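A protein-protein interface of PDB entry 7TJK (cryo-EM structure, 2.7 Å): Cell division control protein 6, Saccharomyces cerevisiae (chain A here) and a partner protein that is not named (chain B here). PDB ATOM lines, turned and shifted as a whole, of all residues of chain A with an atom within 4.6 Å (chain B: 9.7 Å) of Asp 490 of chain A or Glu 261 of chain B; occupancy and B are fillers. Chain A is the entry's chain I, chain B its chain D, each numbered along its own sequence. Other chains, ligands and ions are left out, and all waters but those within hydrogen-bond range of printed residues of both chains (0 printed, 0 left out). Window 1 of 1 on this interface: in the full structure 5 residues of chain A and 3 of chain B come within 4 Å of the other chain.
Asn 258 of chain B touches Arg 458 of chain A. Leu 462 of chain A touches Glu 261 of chain B (CD1 to OE2, 3.7 Å). Glu 261 of chain B touches Lys 478 of chain A. CD1 of Phe 488 of chain A touches CG of Pro 228 of chain B, at 3.7 Å. Asp 490 of chain A touches Glu 261 of chain B (OD2 to O, 3.8 Å).
Of the printed residues of chain B, Asp 490 of chain A touches Glu 261. Of chain A, only Arg 458 (2.4 Å), Leu 462 (3.7 Å), Lys 478 (3.9 Å) and Asp 490 (3.8 Å) come within 4 Å of Glu 261 of chain B. No residue of chain B comes within 4 Å of Thr 435 of chain A. Of the printed residues of chain B, Leu 462 of chain A touches Glu 261. Of the printed residues of chain B, Arg 458 of chain A touches Asn 258 (3.996 Å) and Glu 261 (2.4 Å). Printed residues of chain A within 4 Å of Asn 258 of chain B: Arg 458. Printed residues of chain A within 4 Å of Pro 228 of chain B: Phe 488 (3.7 Å). Leu 257 of chain B touches none of the printed residues of chain A. The nearest printed residue of chain B that does not touch Phe 488 of chain A is Tyr 262 of chain B (6.4 Å).
The side-chain carboxylate (OE2) of Glu 261 of chain B is in salt-bridge range of the guanidinium group (NH1) of Arg 458 of chain A (2.4 Å).
OD2 of Asp 490 of chain A is in salt-bridge range of NZ of Lys 478 of chain A. The backbone NH of Ile 436 of chain A sits at hydrogen-bond distance from the backbone carbonyl oxygen of Asp 490 of chain A (3.1 Å).
Of the 12 printed residues of chain A, 5 touch a printed residue of chain B. Printed residues of chain A that touch a printed residue of chain B: Arg 458, Leu 462, Lys 478, Phe 488 and Asp 490. Along chain A the printed residues that touch a printed residue of chain B span positions 458 to 490. Among the printed residues, Asp or Glu carboxylates within 4 Å of a Lys or Arg side-chain nitrogen of the other chain: Arg 458 of chain A with Glu 261 of chain B (2.4 Å).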
ATOM      1  N   THR A 435     -13.092 -29.682 -43.363  1.00  0.00           N
ATOM      2  CA  THR A 435     -13.636 -29.560 -42.022  1.00  0.00           C
ATOM      3  C   THR A 435     -14.710 -30.620 -41.785  1.00  0.00           C
ATOM      4  O   THR A 435     -15.062 -31.400 -42.675  1.00  0.00           O
ATOM      5  CB  THR A 435     -14.198 -28.157 -41.814  1.00  0.00           C
ATOM      6  OG1 THR A 435     -15.240 -27.915 -42.768  1.00  0.00           O
ATOM      7  CG2 THR A 435     -13.110 -27.116 -42.002  1.00  0.00           C
ATOM      8  N   ILE A 436     -15.231 -30.653 -40.555  1.00  0.00           N
ATOM      9  CA  ILE A 436     -16.330 -31.556 -40.225  1.00  0.00           C
ATOM     10  C   ILE A 436     -17.589 -31.176 -40.996  1.00  0.00           C
ATOM     11  O   ILE A 436     -18.327 -32.052 -41.463  1.00  0.00           O
ATOM     12  CB  ILE A 436     -16.569 -31.564 -38.702  1.00  0.00           C
ATOM     13  CG1 ILE A 436     -15.272 -31.888 -37.962  1.00  0.00           C
ATOM     14  CG2 ILE A 436     -17.640 -32.573 -38.314  1.00  0.00           C
ATOM     15  CD1 ILE A 436     -15.385 -31.778 -36.464  1.00  0.00           C
ATOM     16  N   ARG A 458     -26.617 -32.793 -38.487  1.00  0.00           N
ATOM     17  CA  ARG A 458     -25.203 -32.447 -38.403  1.00  0.00           C
ATOM     18  C   ARG A 458     -24.613 -32.815 -37.046  1.00  0.00           C
ATOM     19  O   ARG A 458     -23.480 -33.306 -36.982  1.00  0.00           O
ATOM     20  CB  ARG A 458     -25.031 -30.952 -38.722  1.00  0.00           C
ATOM     21  CG  ARG A 458     -23.593 -30.400 -38.834  1.00  0.00           C
ATOM     22  CD  ARG A 458     -23.046 -29.845 -37.518  1.00  0.00           C
ATOM     23  NE  ARG A 458     -21.753 -29.193 -37.672  1.00  0.00           N
ATOM     24  CZ  ARG A 458     -20.999 -28.789 -36.660  1.00  0.00           C
ATOM     25  NH1 ARG A 458     -21.376 -28.967 -35.406  1.00  0.00           N
ATOM     26  NH2 ARG A 458     -19.837 -28.194 -36.914  1.00  0.00           N
ATOM     27  N   LEU A 462     -21.591 -35.535 -36.010  1.00  0.00           N
ATOM     28  CA  LEU A 462     -20.409 -35.283 -35.193  1.00  0.00           C
ATOM     29  C   LEU A 462     -20.342 -36.230 -34.000  1.00  0.00           C
ATOM     30  O   LEU A 462     -19.252 -36.490 -33.481  1.00  0.00           O
ATOM     31  CB  LEU A 462     -20.401 -33.812 -34.749  1.00  0.00           C
ATOM     32  CG  LEU A 462     -19.235 -33.126 -34.018  1.00  0.00           C
ATOM     33  CD1 LEU A 462     -19.274 -31.642 -34.331  1.00  0.00           C
ATOM     34  CD2 LEU A 462     -19.276 -33.301 -32.504  1.00  0.00           C
ATOM     35  N   ILE A 476      -9.409 -36.383 -34.437  1.00  0.00           N
ATOM     36  CA  ILE A 476      -9.937 -35.035 -34.631  1.00  0.00           C
ATOM     37  C   ILE A 476      -8.958 -34.008 -34.072  1.00  0.00           C
ATOM     38  O   ILE A 476      -8.594 -34.062 -32.892  1.00  0.00           O
ATOM     39  CB  ILE A 476     -11.316 -34.890 -33.965  1.00  0.00           C
ATOM     40  CG1 ILE A 476     -12.343 -35.767 -34.673  1.00  0.00           C
ATOM     41  CG2 ILE A 476     -11.784 -33.444 -33.984  1.00  0.00           C
ATOM     42  CD1 ILE A 476     -13.676 -35.852 -33.963  1.00  0.00           C
ATOM     43  N   LYS A 477      -8.537 -33.065 -34.916  1.00  0.00           N
ATOM     44  CA  LYS A 477      -7.703 -31.944 -34.500  1.00  0.00           C
ATOM     45  C   LYS A 477      -8.373 -30.615 -34.825  1.00  0.00           C
ATOM     46  O   LYS A 477      -9.300 -30.531 -35.636  1.00  0.00           O
ATOM     47  CB  LYS A 477      -6.311 -31.963 -35.151  1.00  0.00           C
ATOM     48  CG  LYS A 477      -5.270 -32.885 -34.532  1.00  0.00           C
ATOM     49  CD  LYS A 477      -5.465 -34.362 -34.786  1.00  0.00           C
ATOM     50  CE  LYS A 477      -4.291 -35.117 -34.184  1.00  0.00           C
ATOM     51  NZ  LYS A 477      -4.410 -36.591 -34.264  1.00  0.00           N
ATOM     52  N   LYS A 478      -7.883 -29.569 -34.163  1.00  0.00           N
ATOM     53  CA  LYS A 478      -8.268 -28.187 -34.429  1.00  0.00           C
ATOM     54  C   LYS A 478      -7.037 -27.442 -34.925  1.00  0.00           C
ATOM     55  O   LYS A 478      -6.100 -27.206 -34.157  1.00  0.00           O
ATOM     56  CB  LYS A 478      -8.833 -27.524 -33.175  1.00  0.00           C
ATOM     57  CG  LYS A 478      -9.335 -26.116 -33.404  1.00  0.00           C
ATOM     58  CD  LYS A 478     -10.707 -25.911 -32.801  1.00  0.00           C
ATOM     59  CE  LYS A 478     -11.119 -24.458 -32.908  1.00  0.00           C
ATOM     60  NZ  LYS A 478     -12.310 -24.169 -32.070  1.00  0.00           N
ATOM     61  N   PHE A 488      -9.597 -20.699 -36.860  1.00  0.00           N
ATOM     62  CA  PHE A 488      -9.372 -22.052 -36.372  1.00  0.00           C
ATOM     63  C   PHE A 488     -10.615 -22.896 -36.623  1.00  0.00           C
ATOM     64  O   PHE A 488     -11.725 -22.510 -36.241  1.00  0.00           O
ATOM     65  CB  PHE A 488      -9.013 -22.033 -34.888  1.00  0.00           C
ATOM     66  CG  PHE A 488      -7.564 -21.764 -34.630  1.00  0.00           C
ATOM     67  CD1 PHE A 488      -7.102 -20.462 -34.490  1.00  0.00           C
ATOM     68  CD2 PHE A 488      -6.657 -22.811 -34.536  1.00  0.00           C
ATOM     69  CE1 PHE A 488      -5.767 -20.209 -34.257  1.00  0.00           C
ATOM     70  CE2 PHE A 488      -5.320 -22.566 -34.307  1.00  0.00           C
ATOM     71  CZ  PHE A 488      -4.873 -21.261 -34.165  1.00  0.00           C
ATOM     72  N   VAL A 489     -10.426 -24.043 -37.273  1.00  0.00           N
ATOM     73  CA  VAL A 489     -11.518 -24.937 -37.635  1.00  0.00           C
ATOM     74  C   VAL A 489     -11.186 -26.343 -37.161  1.00  0.00           C
ATOM     75  O   VAL A 489     -10.023 -26.685 -36.921  1.00  0.00           O
ATOM     76  CB  VAL A 489     -11.798 -24.934 -39.156  1.00  0.00           C
ATOM     77  CG1 VAL A 489     -12.381 -23.601 -39.594  1.00  0.00           C
ATOM     78  CG2 VAL A 489     -10.529 -25.237 -39.928  1.00  0.00           C
ATOM     79  N   ASP A 490     -12.225 -27.158 -37.019  1.00  0.00           N
ATOM     80  CA  ASP A 490     -12.077 -28.551 -36.624  1.00  0.00           C
ATOM     81  C   ASP A 490     -12.195 -29.436 -37.857  1.00  0.00           C
ATOM     82  O   ASP A 490     -13.155 -29.314 -38.624  1.00  0.00           O
ATOM     83  CB  ASP A 490     -13.136 -28.927 -35.589  1.00  0.00           C
ATOM     84  CG  ASP A 490     -12.779 -28.464 -34.192  1.00  0.00           C
ATOM     85  OD1 ASP A 490     -11.794 -28.982 -33.624  1.00  0.00           O
ATOM     86  OD2 ASP A 490     -13.489 -27.589 -33.655  1.00  0.00           O
ATOM     87  N   LYS A 491     -11.218 -30.318 -38.050  1.00  0.00           N
ATOM     88  CA  LYS A 491     -11.160 -31.128 -39.255  1.00  0.00           C
ATOM     89  C   LYS A 491     -10.786 -32.562 -38.915  1.00  0.00           C
ATOM     90  O   LYS A 491     -10.110 -32.841 -37.922  1.00  0.00           O
ATOM     91  CB  LYS A 491     -10.184 -30.535 -40.279  1.00  0.00           C
ATOM     92  CG  LYS A 491      -8.739 -30.498 -39.850  1.00  0.00           C
ATOM     93  CD  LYS A 491      -7.941 -29.666 -40.832  1.00  0.00           C
ATOM     94  CE  LYS A 491      -8.410 -28.219 -40.816  1.00  0.00           C
ATOM     95  NZ  LYS A 491      -7.695 -27.386 -41.820  1.00  0.00           N
ATOM     96  N   ILE A 492     -11.246 -33.472 -39.771  1.00  0.00           N
ATOM     97  CA  ILE A 492     -11.140 -34.911 -39.566  1.00  0.00           C
ATOM     98  C   ILE A 492      -9.852 -35.412 -40.208  1.00  0.00           C
ATOM     99  O   ILE A 492      -9.546 -35.071 -41.356  1.00  0.00           O
ATOM    100  CB  ILE A 492     -12.366 -35.628 -40.167  1.00  0.00           C
ATOM    101  CG1 ILE A 492     -13.665 -35.122 -39.535  1.00  0.00           C
ATOM    102  CG2 ILE A 492     -12.267 -37.121 -39.968  1.00  0.00           C
ATOM    103  CD1 ILE A 492     -13.766 -35.350 -38.056  1.00  0.00           C
ATOM    104  N   ILE B 102     -23.910 -21.781 -20.007  1.00  0.00           N
ATOM    105  CA  ILE B 102     -23.560 -20.782 -21.008  1.00  0.00           C
ATOM    106  C   ILE B 102     -24.837 -20.324 -21.702  1.00  0.00           C
ATOM    107  O   ILE B 102     -25.612 -21.146 -22.202  1.00  0.00           O
ATOM    108  CB  ILE B 102     -22.539 -21.333 -22.020  1.00  0.00           C
ATOM    109  CG1 ILE B 102     -21.246 -21.725 -21.303  1.00  0.00           C
ATOM    110  CG2 ILE B 102     -22.248 -20.313 -23.105  1.00  0.00           C
ATOM    111  CD1 ILE B 102     -20.252 -22.440 -22.180  1.00  0.00           C
ATOM    112  N   VAL B 104     -26.278 -18.509 -24.880  1.00  0.00           N
ATOM    113  CA  VAL B 104     -25.903 -18.281 -26.266  1.00  0.00           C
ATOM    114  C   VAL B 104     -27.007 -17.470 -26.925  1.00  0.00           C
ATOM    115  O   VAL B 104     -28.166 -17.896 -26.964  1.00  0.00           O
ATOM    116  CB  VAL B 104     -25.667 -19.601 -27.012  1.00  0.00           C
ATOM    117  CG1 VAL B 104     -25.344 -19.333 -28.468  1.00  0.00           C
ATOM    118  CG2 VAL B 104     -24.556 -20.380 -26.352  1.00  0.00           C
ATOM    119  N   ASP B 223     -16.274 -17.042 -25.054  1.00  0.00           N
ATOM    120  CA  ASP B 223     -15.612 -17.589 -26.233  1.00  0.00           C
ATOM    121  C   ASP B 223     -14.170 -17.110 -26.362  1.00  0.00           C
ATOM    122  O   ASP B 223     -13.342 -17.811 -26.953  1.00  0.00           O
ATOM    123  CB  ASP B 223     -16.403 -17.221 -27.486  1.00  0.00           C
ATOM    124  CG  ASP B 223     -16.675 -15.733 -27.586  1.00  0.00           C
ATOM    125  OD1 ASP B 223     -17.563 -15.239 -26.860  1.00  0.00           O
ATOM    126  OD2 ASP B 223     -16.001 -15.055 -28.388  1.00  0.00           O
ATOM    127  N   ALA B 226     -12.039 -19.543 -24.510  1.00  0.00           N
ATOM    128  CA  ALA B 226     -12.009 -20.883 -25.090  1.00  0.00           C
ATOM    129  C   ALA B 226     -11.137 -20.924 -26.341  1.00  0.00           C
ATOM    130  O   ALA B 226     -11.571 -21.342 -27.412  1.00  0.00           O
ATOM    131  CB  ALA B 226     -13.426 -21.353 -25.389  1.00  0.00           C
ATOM    132  N   GLY B 227      -9.891 -20.482 -26.204  1.00  0.00           N
ATOM    133  CA  GLY B 227      -8.974 -20.425 -27.318  1.00  0.00           C
ATOM    134  C   GLY B 227      -8.432 -21.789 -27.680  1.00  0.00           C
ATOM    135  O   GLY B 227      -8.585 -22.779 -26.951  1.00  0.00           O
ATOM    136  N   PRO B 228      -7.775 -21.861 -28.840  1.00  0.00           N
ATOM    137  CA  PRO B 228      -7.272 -23.150 -29.327  1.00  0.00           C
ATOM    138  C   PRO B 228      -5.900 -23.533 -28.800  1.00  0.00           C
ATOM    139  O   PRO B 228      -5.358 -24.554 -29.237  1.00  0.00           O
ATOM    140  CB  PRO B 228      -7.234 -22.938 -30.844  1.00  0.00           C
ATOM    141  CG  PRO B 228      -6.905 -21.500 -30.982  1.00  0.00           C
ATOM    142  CD  PRO B 228      -7.590 -20.793 -29.839  1.00  0.00           C
ATOM    143  N   GLN B 231      -6.578 -23.443 -22.051  1.00  0.00           N
ATOM    144  CA  GLN B 231      -7.812 -22.945 -21.446  1.00  0.00           C
ATOM    145  C   GLN B 231      -7.774 -23.108 -19.931  1.00  0.00           C
ATOM    146  O   GLN B 231      -8.654 -23.734 -19.336  1.00  0.00           O
ATOM    147  CB  GLN B 231      -9.026 -23.655 -22.039  1.00  0.00           C
ATOM    148  CG  GLN B 231      -9.243 -23.380 -23.519  1.00  0.00           C
ATOM    149  CD  GLN B 231     -10.439 -24.118 -24.084  1.00  0.00           C
ATOM    150  OE1 GLN B 231     -11.295 -24.593 -23.344  1.00  0.00           O
ATOM    151  NE2 GLN B 231     -10.501 -24.218 -25.402  1.00  0.00           N
ATOM    152  N   LYS B 256     -21.422 -16.997 -29.908  1.00  0.00           N
ATOM    153  CA  LYS B 256     -21.053 -18.114 -30.768  1.00  0.00           C
ATOM    154  C   LYS B 256     -22.039 -19.263 -30.593  1.00  0.00           C
ATOM    155  O   LYS B 256     -22.214 -19.773 -29.481  1.00  0.00           O
ATOM    156  CB  LYS B 256     -19.634 -18.571 -30.448  1.00  0.00           C
ATOM    157  CG  LYS B 256     -18.579 -17.499 -30.632  1.00  0.00           C
ATOM    158  CD  LYS B 256     -18.530 -17.021 -32.071  1.00  0.00           C
ATOM    159  CE  LYS B 256     -17.866 -15.662 -32.183  1.00  0.00           C
ATOM    160  NZ  LYS B 256     -17.809 -15.196 -33.592  1.00  0.00           N
ATOM    161  N   LEU B 257     -22.680 -19.662 -31.695  1.00  0.00           N
ATOM    162  CA  LEU B 257     -23.657 -20.746 -31.659  1.00  0.00           C
ATOM    163  C   LEU B 257     -23.007 -22.083 -31.324  1.00  0.00           C
ATOM    164  O   LEU B 257     -23.558 -22.867 -30.544  1.00  0.00           O
ATOM    165  CB  LEU B 257     -24.387 -20.833 -33.000  1.00  0.00           C
ATOM    166  CG  LEU B 257     -25.437 -19.768 -33.313  1.00  0.00           C
ATOM    167  CD1 LEU B 257     -25.984 -19.974 -34.709  1.00  0.00           C
ATOM    168  CD2 LEU B 257     -26.556 -19.799 -32.293  1.00  0.00           C
ATOM    169  N   ASN B 258     -21.844 -22.363 -31.900  1.00  0.00           N
ATOM    170  CA  ASN B 258     -21.142 -23.624 -31.657  1.00  0.00           C
ATOM    171  C   ASN B 258     -20.097 -23.461 -30.553  1.00  0.00           C
ATOM    172  O   ASN B 258     -18.914 -23.721 -30.739  1.00  0.00           O
ATOM    173  CB  ASN B 258     -20.509 -24.130 -32.950  1.00  0.00           C
ATOM    174  CG  ASN B 258     -21.538 -24.462 -34.010  1.00  0.00           C
ATOM    175  OD1 ASN B 258     -21.598 -23.819 -35.058  1.00  0.00           O
ATOM    176  ND2 ASN B 258     -22.360 -25.470 -33.742  1.00  0.00           N
ATOM    177  N   ILE B 259     -20.568 -23.037 -29.377  1.00  0.00           N
ATOM    178  CA  ILE B 259     -19.672 -22.760 -28.255  1.00  0.00           C
ATOM    179  C   ILE B 259     -19.094 -24.037 -27.641  1.00  0.00           C
ATOM    180  O   ILE B 259     -17.987 -24.001 -27.091  1.00  0.00           O
ATOM    181  CB  ILE B 259     -20.416 -21.880 -27.223  1.00  0.00           C
ATOM    182  CG1 ILE B 259     -19.464 -21.295 -26.171  1.00  0.00           C
ATOM    183  CG2 ILE B 259     -21.558 -22.636 -26.554  1.00  0.00           C
ATOM    184  CD1 ILE B 259     -18.323 -20.493 -26.745  1.00  0.00           C
ATOM    185  N   LEU B 260     -19.782 -25.179 -27.758  1.00  0.00           N
ATOM    186  CA  LEU B 260     -19.277 -26.409 -27.151  1.00  0.00           C
ATOM    187  C   LEU B 260     -18.090 -26.983 -27.913  1.00  0.00           C
ATOM    188  O   LEU B 260     -17.283 -27.715 -27.330  1.00  0.00           O
ATOM    189  CB  LEU B 260     -20.387 -27.453 -27.053  1.00  0.00           C
ATOM    190  CG  LEU B 260     -21.552 -27.143 -26.119  1.00  0.00           C
ATOM    191  CD1 LEU B 260     -22.623 -28.212 -26.244  1.00  0.00           C
ATOM    192  CD2 LEU B 260     -21.068 -27.024 -24.688  1.00  0.00           C
ATOM    193  N   GLU B 261     -17.964 -26.674 -29.204  1.00  0.00           N
ATOM    194  CA  GLU B 261     -16.812 -27.114 -29.978  1.00  0.00           C
ATOM    195  C   GLU B 261     -15.572 -26.269 -29.721  1.00  0.00           C
ATOM    196  O   GLU B 261     -14.469 -26.690 -30.085  1.00  0.00           O
ATOM    197  CB  GLU B 261     -17.140 -27.103 -31.471  1.00  0.00           C
ATOM    198  CG  GLU B 261     -18.472 -27.742 -31.819  1.00  0.00           C
ATOM    199  CD  GLU B 261     -18.835 -27.568 -33.278  1.00  0.00           C
ATOM    200  OE1 GLU B 261     -18.062 -26.914 -34.010  1.00  0.00           O
ATOM    201  OE2 GLU B 261     -19.892 -28.082 -33.695  1.00  0.00           O
ATOM    202  N   TYR B 262     -15.730 -25.095 -29.111  1.00  0.00           N
ATOM    203  CA  TYR B 262     -14.604 -24.255 -28.726  1.00  0.00           C
ATOM    204  C   TYR B 262     -13.829 -24.824 -27.546  1.00  0.00           C
ATOM    205  O   TYR B 262     -12.628 -24.566 -27.428  1.00  0.00           O
ATOM    206  CB  TYR B 262     -15.099 -22.850 -28.367  1.00  0.00           C
ATOM    207  CG  TYR B 262     -15.297 -21.898 -29.529  1.00  0.00           C
ATOM    208  CD1 TYR B 262     -16.088 -22.245 -30.617  1.00  0.00           C
ATOM    209  CD2 TYR B 262     -14.717 -20.636 -29.517  1.00  0.00           C
ATOM    210  CE1 TYR B 262     -16.278 -21.373 -31.671  1.00  0.00           C
ATOM    211  CE2 TYR B 262     -14.903 -19.755 -30.564  1.00  0.00           C
ATOM    212  CZ  TYR B 262     -15.685 -20.131 -31.641  1.00  0.00           C
ATOM    213  OH  TYR B 262     -15.874 -19.262 -32.689  1.00  0.00           O
ATOM    214  N   LEU B 263     -14.488 -25.586 -26.680  1.00  0.00           N
ATOM    215  CA  LEU B 263     -13.894 -26.042 -25.434  1.00  0.00           C
ATOM    216  C   LEU B 263     -12.921 -27.194 -25.663  1.00  0.00           C
ATOM    217  O   LEU B 263     -13.117 -28.039 -26.540  1.00  0.00           O
ATOM    218  CB  LEU B 263     -14.990 -26.471 -24.457  1.00  0.00           C
ATOM    219  CG  LEU B 263     -16.016 -25.393 -24.094  1.00  0.00           C
ATOM    220  CD1 LEU B 263     -17.207 -25.983 -23.356  1.00  0.00           C
ATOM    221  CD2 LEU B 263     -15.371 -24.288 -23.273  1.00  0.00           C
ATOM    222  N   GLU B 264     -11.860 -27.211 -24.861  1.00  0.00           N
ATOM    223  CA  GLU B 264     -10.926 -28.325 -24.824  1.00  0.00           C
ATOM    224  C   GLU B 264     -11.616 -29.525 -24.172  1.00  0.00           C
ATOM    225  O   GLU B 264     -12.588 -29.368 -23.431  1.00  0.00           O
ATOM    226  CB  GLU B 264      -9.656 -27.895 -24.073  1.00  0.00           C
ATOM    227  CG  GLU B 264      -8.443 -28.834 -24.108  1.00  0.00           C
ATOM    228  CD  GLU B 264      -8.433 -29.844 -22.977  1.00  0.00           C
ATOM    229  OE1 GLU B 264      -8.510 -29.422 -21.804  1.00  0.00           O
ATOM    230  OE2 GLU B 264      -8.336 -31.055 -23.259  1.00  0.00           O
ATOM    231  N   LYS B 265     -11.107 -30.731 -24.474  1.00  0.00           N
ATOM    232  CA  LYS B 265     -11.777 -31.983 -24.103  1.00  0.00           C
ATOM    233  C   LYS B 265     -11.936 -32.137 -22.593  1.00  0.00           C
ATOM    234  O   LYS B 265     -12.988 -32.577 -22.121  1.00  0.00           O
ATOM    235  CB  LYS B 265     -11.008 -33.179 -24.663  1.00  0.00           C
ATOM    236  CG  LYS B 265     -11.043 -33.322 -26.169  1.00  0.00           C
ATOM    237  CD  LYS B 265     -10.187 -34.497 -26.611  1.00  0.00           C
ATOM    238  CE  LYS B 265     -10.819 -35.825 -26.219  1.00  0.00           C
ATOM    239  NZ  LYS B 265     -12.075 -36.094 -26.972  1.00  0.00           N
ATOM    240  N   VAL B 267     -11.867 -29.583 -20.404  1.00  0.00           N
ATOM    241  CA  VAL B 267     -12.780 -28.500 -20.051  1.00  0.00           C
ATOM    242  C   VAL B 267     -14.216 -28.874 -20.401  1.00  0.00           C
ATOM    243  O   VAL B 267     -15.143 -28.640 -19.617  1.00  0.00           O
ATOM    244  CB  VAL B 267     -12.330 -27.203 -20.752  1.00  0.00           C
ATOM    245  CG1 VAL B 267     -13.333 -26.081 -20.556  1.00  0.00           C
ATOM    246  CG2 VAL B 267     -10.960 -26.784 -20.251  1.00  0.00           C
ATOM    247  N   LYS B 268     -14.414 -29.484 -21.575  1.00  0.00           N
ATOM    248  CA  LYS B 268     -15.733 -29.951 -21.989  1.00  0.00           C
ATOM    249  C   LYS B 268     -16.238 -31.082 -21.099  1.00  0.00           C
ATOM    250  O   LYS B 268     -17.447 -31.201 -20.874  1.00  0.00           O
ATOM    251  CB  LYS B 268     -15.674 -30.397 -23.452  1.00  0.00           C
ATOM    252  CG  LYS B 268     -17.003 -30.616 -24.123  1.00  0.00           C
ATOM    253  CD  LYS B 268     -16.866 -31.462 -25.373  1.00  0.00           C
ATOM    254  CE  LYS B 268     -18.210 -31.644 -26.057  1.00  0.00           C
ATOM    255  NZ  LYS B 268     -18.340 -30.764 -27.247  1.00  0.00           N
ATOM    256  N   PHE B 271     -17.366 -29.361 -17.904  1.00  0.00           N
ATOM    257  CA  PHE B 271     -18.536 -28.520 -18.101  1.00  0.00           C
ATOM    258  C   PHE B 271     -19.806 -29.362 -18.014  1.00  0.00           C
ATOM    259  O   PHE B 271     -19.838 -30.523 -18.426  1.00  0.00           O
ATOM    260  CB  PHE B 271     -18.450 -27.800 -19.449  1.00  0.00           C
ATOM    261  CG  PHE B 271     -19.598 -26.873 -19.723  1.00  0.00           C
ATOM    262  CD1 PHE B 271     -19.949 -25.893 -18.808  1.00  0.00           C
ATOM    263  CD2 PHE B 271     -20.325 -26.979 -20.898  1.00  0.00           C
ATOM    264  CE1 PHE B 271     -21.009 -25.039 -19.057  1.00  0.00           C
ATOM    265  CE2 PHE B 271     -21.385 -26.127 -21.152  1.00  0.00           C
ATOM    266  CZ  PHE B 271     -21.727 -25.158 -20.228  1.00  0.00           C
ATOM    267  N   GLN B 273     -22.537 -29.169 -19.604  1.00  0.00           N
ATOM    268  CA  GLN B 273     -23.197 -29.325 -20.908  1.00  0.00           C
ATOM    269  C   GLN B 273     -24.599 -28.729 -20.920  1.00  0.00           C
ATOM    270  O   GLN B 273     -25.471 -29.177 -21.665  1.00  0.00           O
ATOM    271  CB  GLN B 273     -23.241 -30.789 -21.364  1.00  0.00           C
ATOM    272  CG  GLN B 273     -21.877 -31.368 -21.585  1.00  0.00           C
ATOM    273  CD  GLN B 273     -21.168 -30.708 -22.730  1.00  0.00           C
ATOM    274  OE1 GLN B 273     -21.770 -30.388 -23.756  1.00  0.00           O
ATOM    275  NE2 GLN B 273     -19.891 -30.444 -22.543  1.00  0.00           N
ATOM    276  N   VAL B 275     -26.596 -25.657 -21.970  1.00  0.00           N
ATOM    277  CA  VAL B 275     -26.513 -24.499 -22.854  1.00  0.00           C
ATOM    278  C   VAL B 275     -27.919 -23.953 -23.045  1.00  0.00           C
ATOM    279  O   VAL B 275     -28.823 -24.687 -23.461  1.00  0.00           O
ATOM    280  CB  VAL B 275     -25.875 -24.859 -24.207  1.00  0.00           C
ATOM    281  CG1 VAL B 275     -25.866 -23.657 -25.127  1.00  0.00           C
ATOM    282  CG2 VAL B 275     -24.466 -25.392 -24.012  1.00  0.00           C
ATOM    283  N   TYR B 277     -30.100 -21.346 -25.129  1.00  0.00           N
ATOM    284  CA  TYR B 277     -30.166 -20.490 -26.302  1.00  0.00           C
ATOM    285  C   TYR B 277     -31.255 -19.449 -26.096  1.00  0.00           C
ATOM    286  O   TYR B 277     -32.393 -19.794 -25.758  1.00  0.00           O
ATOM    287  CB  TYR B 277     -30.426 -21.316 -27.563  1.00  0.00           C
ATOM    288  CG  TYR B 277     -29.279 -22.236 -27.908  1.00  0.00           C
ATOM    289  CD1 TYR B 277     -28.154 -21.755 -28.563  1.00  0.00           C
ATOM    290  CD2 TYR B 277     -29.312 -23.581 -27.559  1.00  0.00           C
ATOM    291  CE1 TYR B 277     -27.095 -22.586 -28.872  1.00  0.00           C
ATOM    292  CE2 TYR B 277     -28.258 -24.424 -27.865  1.00  0.00           C
ATOM    293  CZ  TYR B 277     -27.153 -23.919 -28.521  1.00  0.00           C
ATOM    294  OH  TYR B 277     -26.101 -24.747 -28.830  1.00  0.00           O
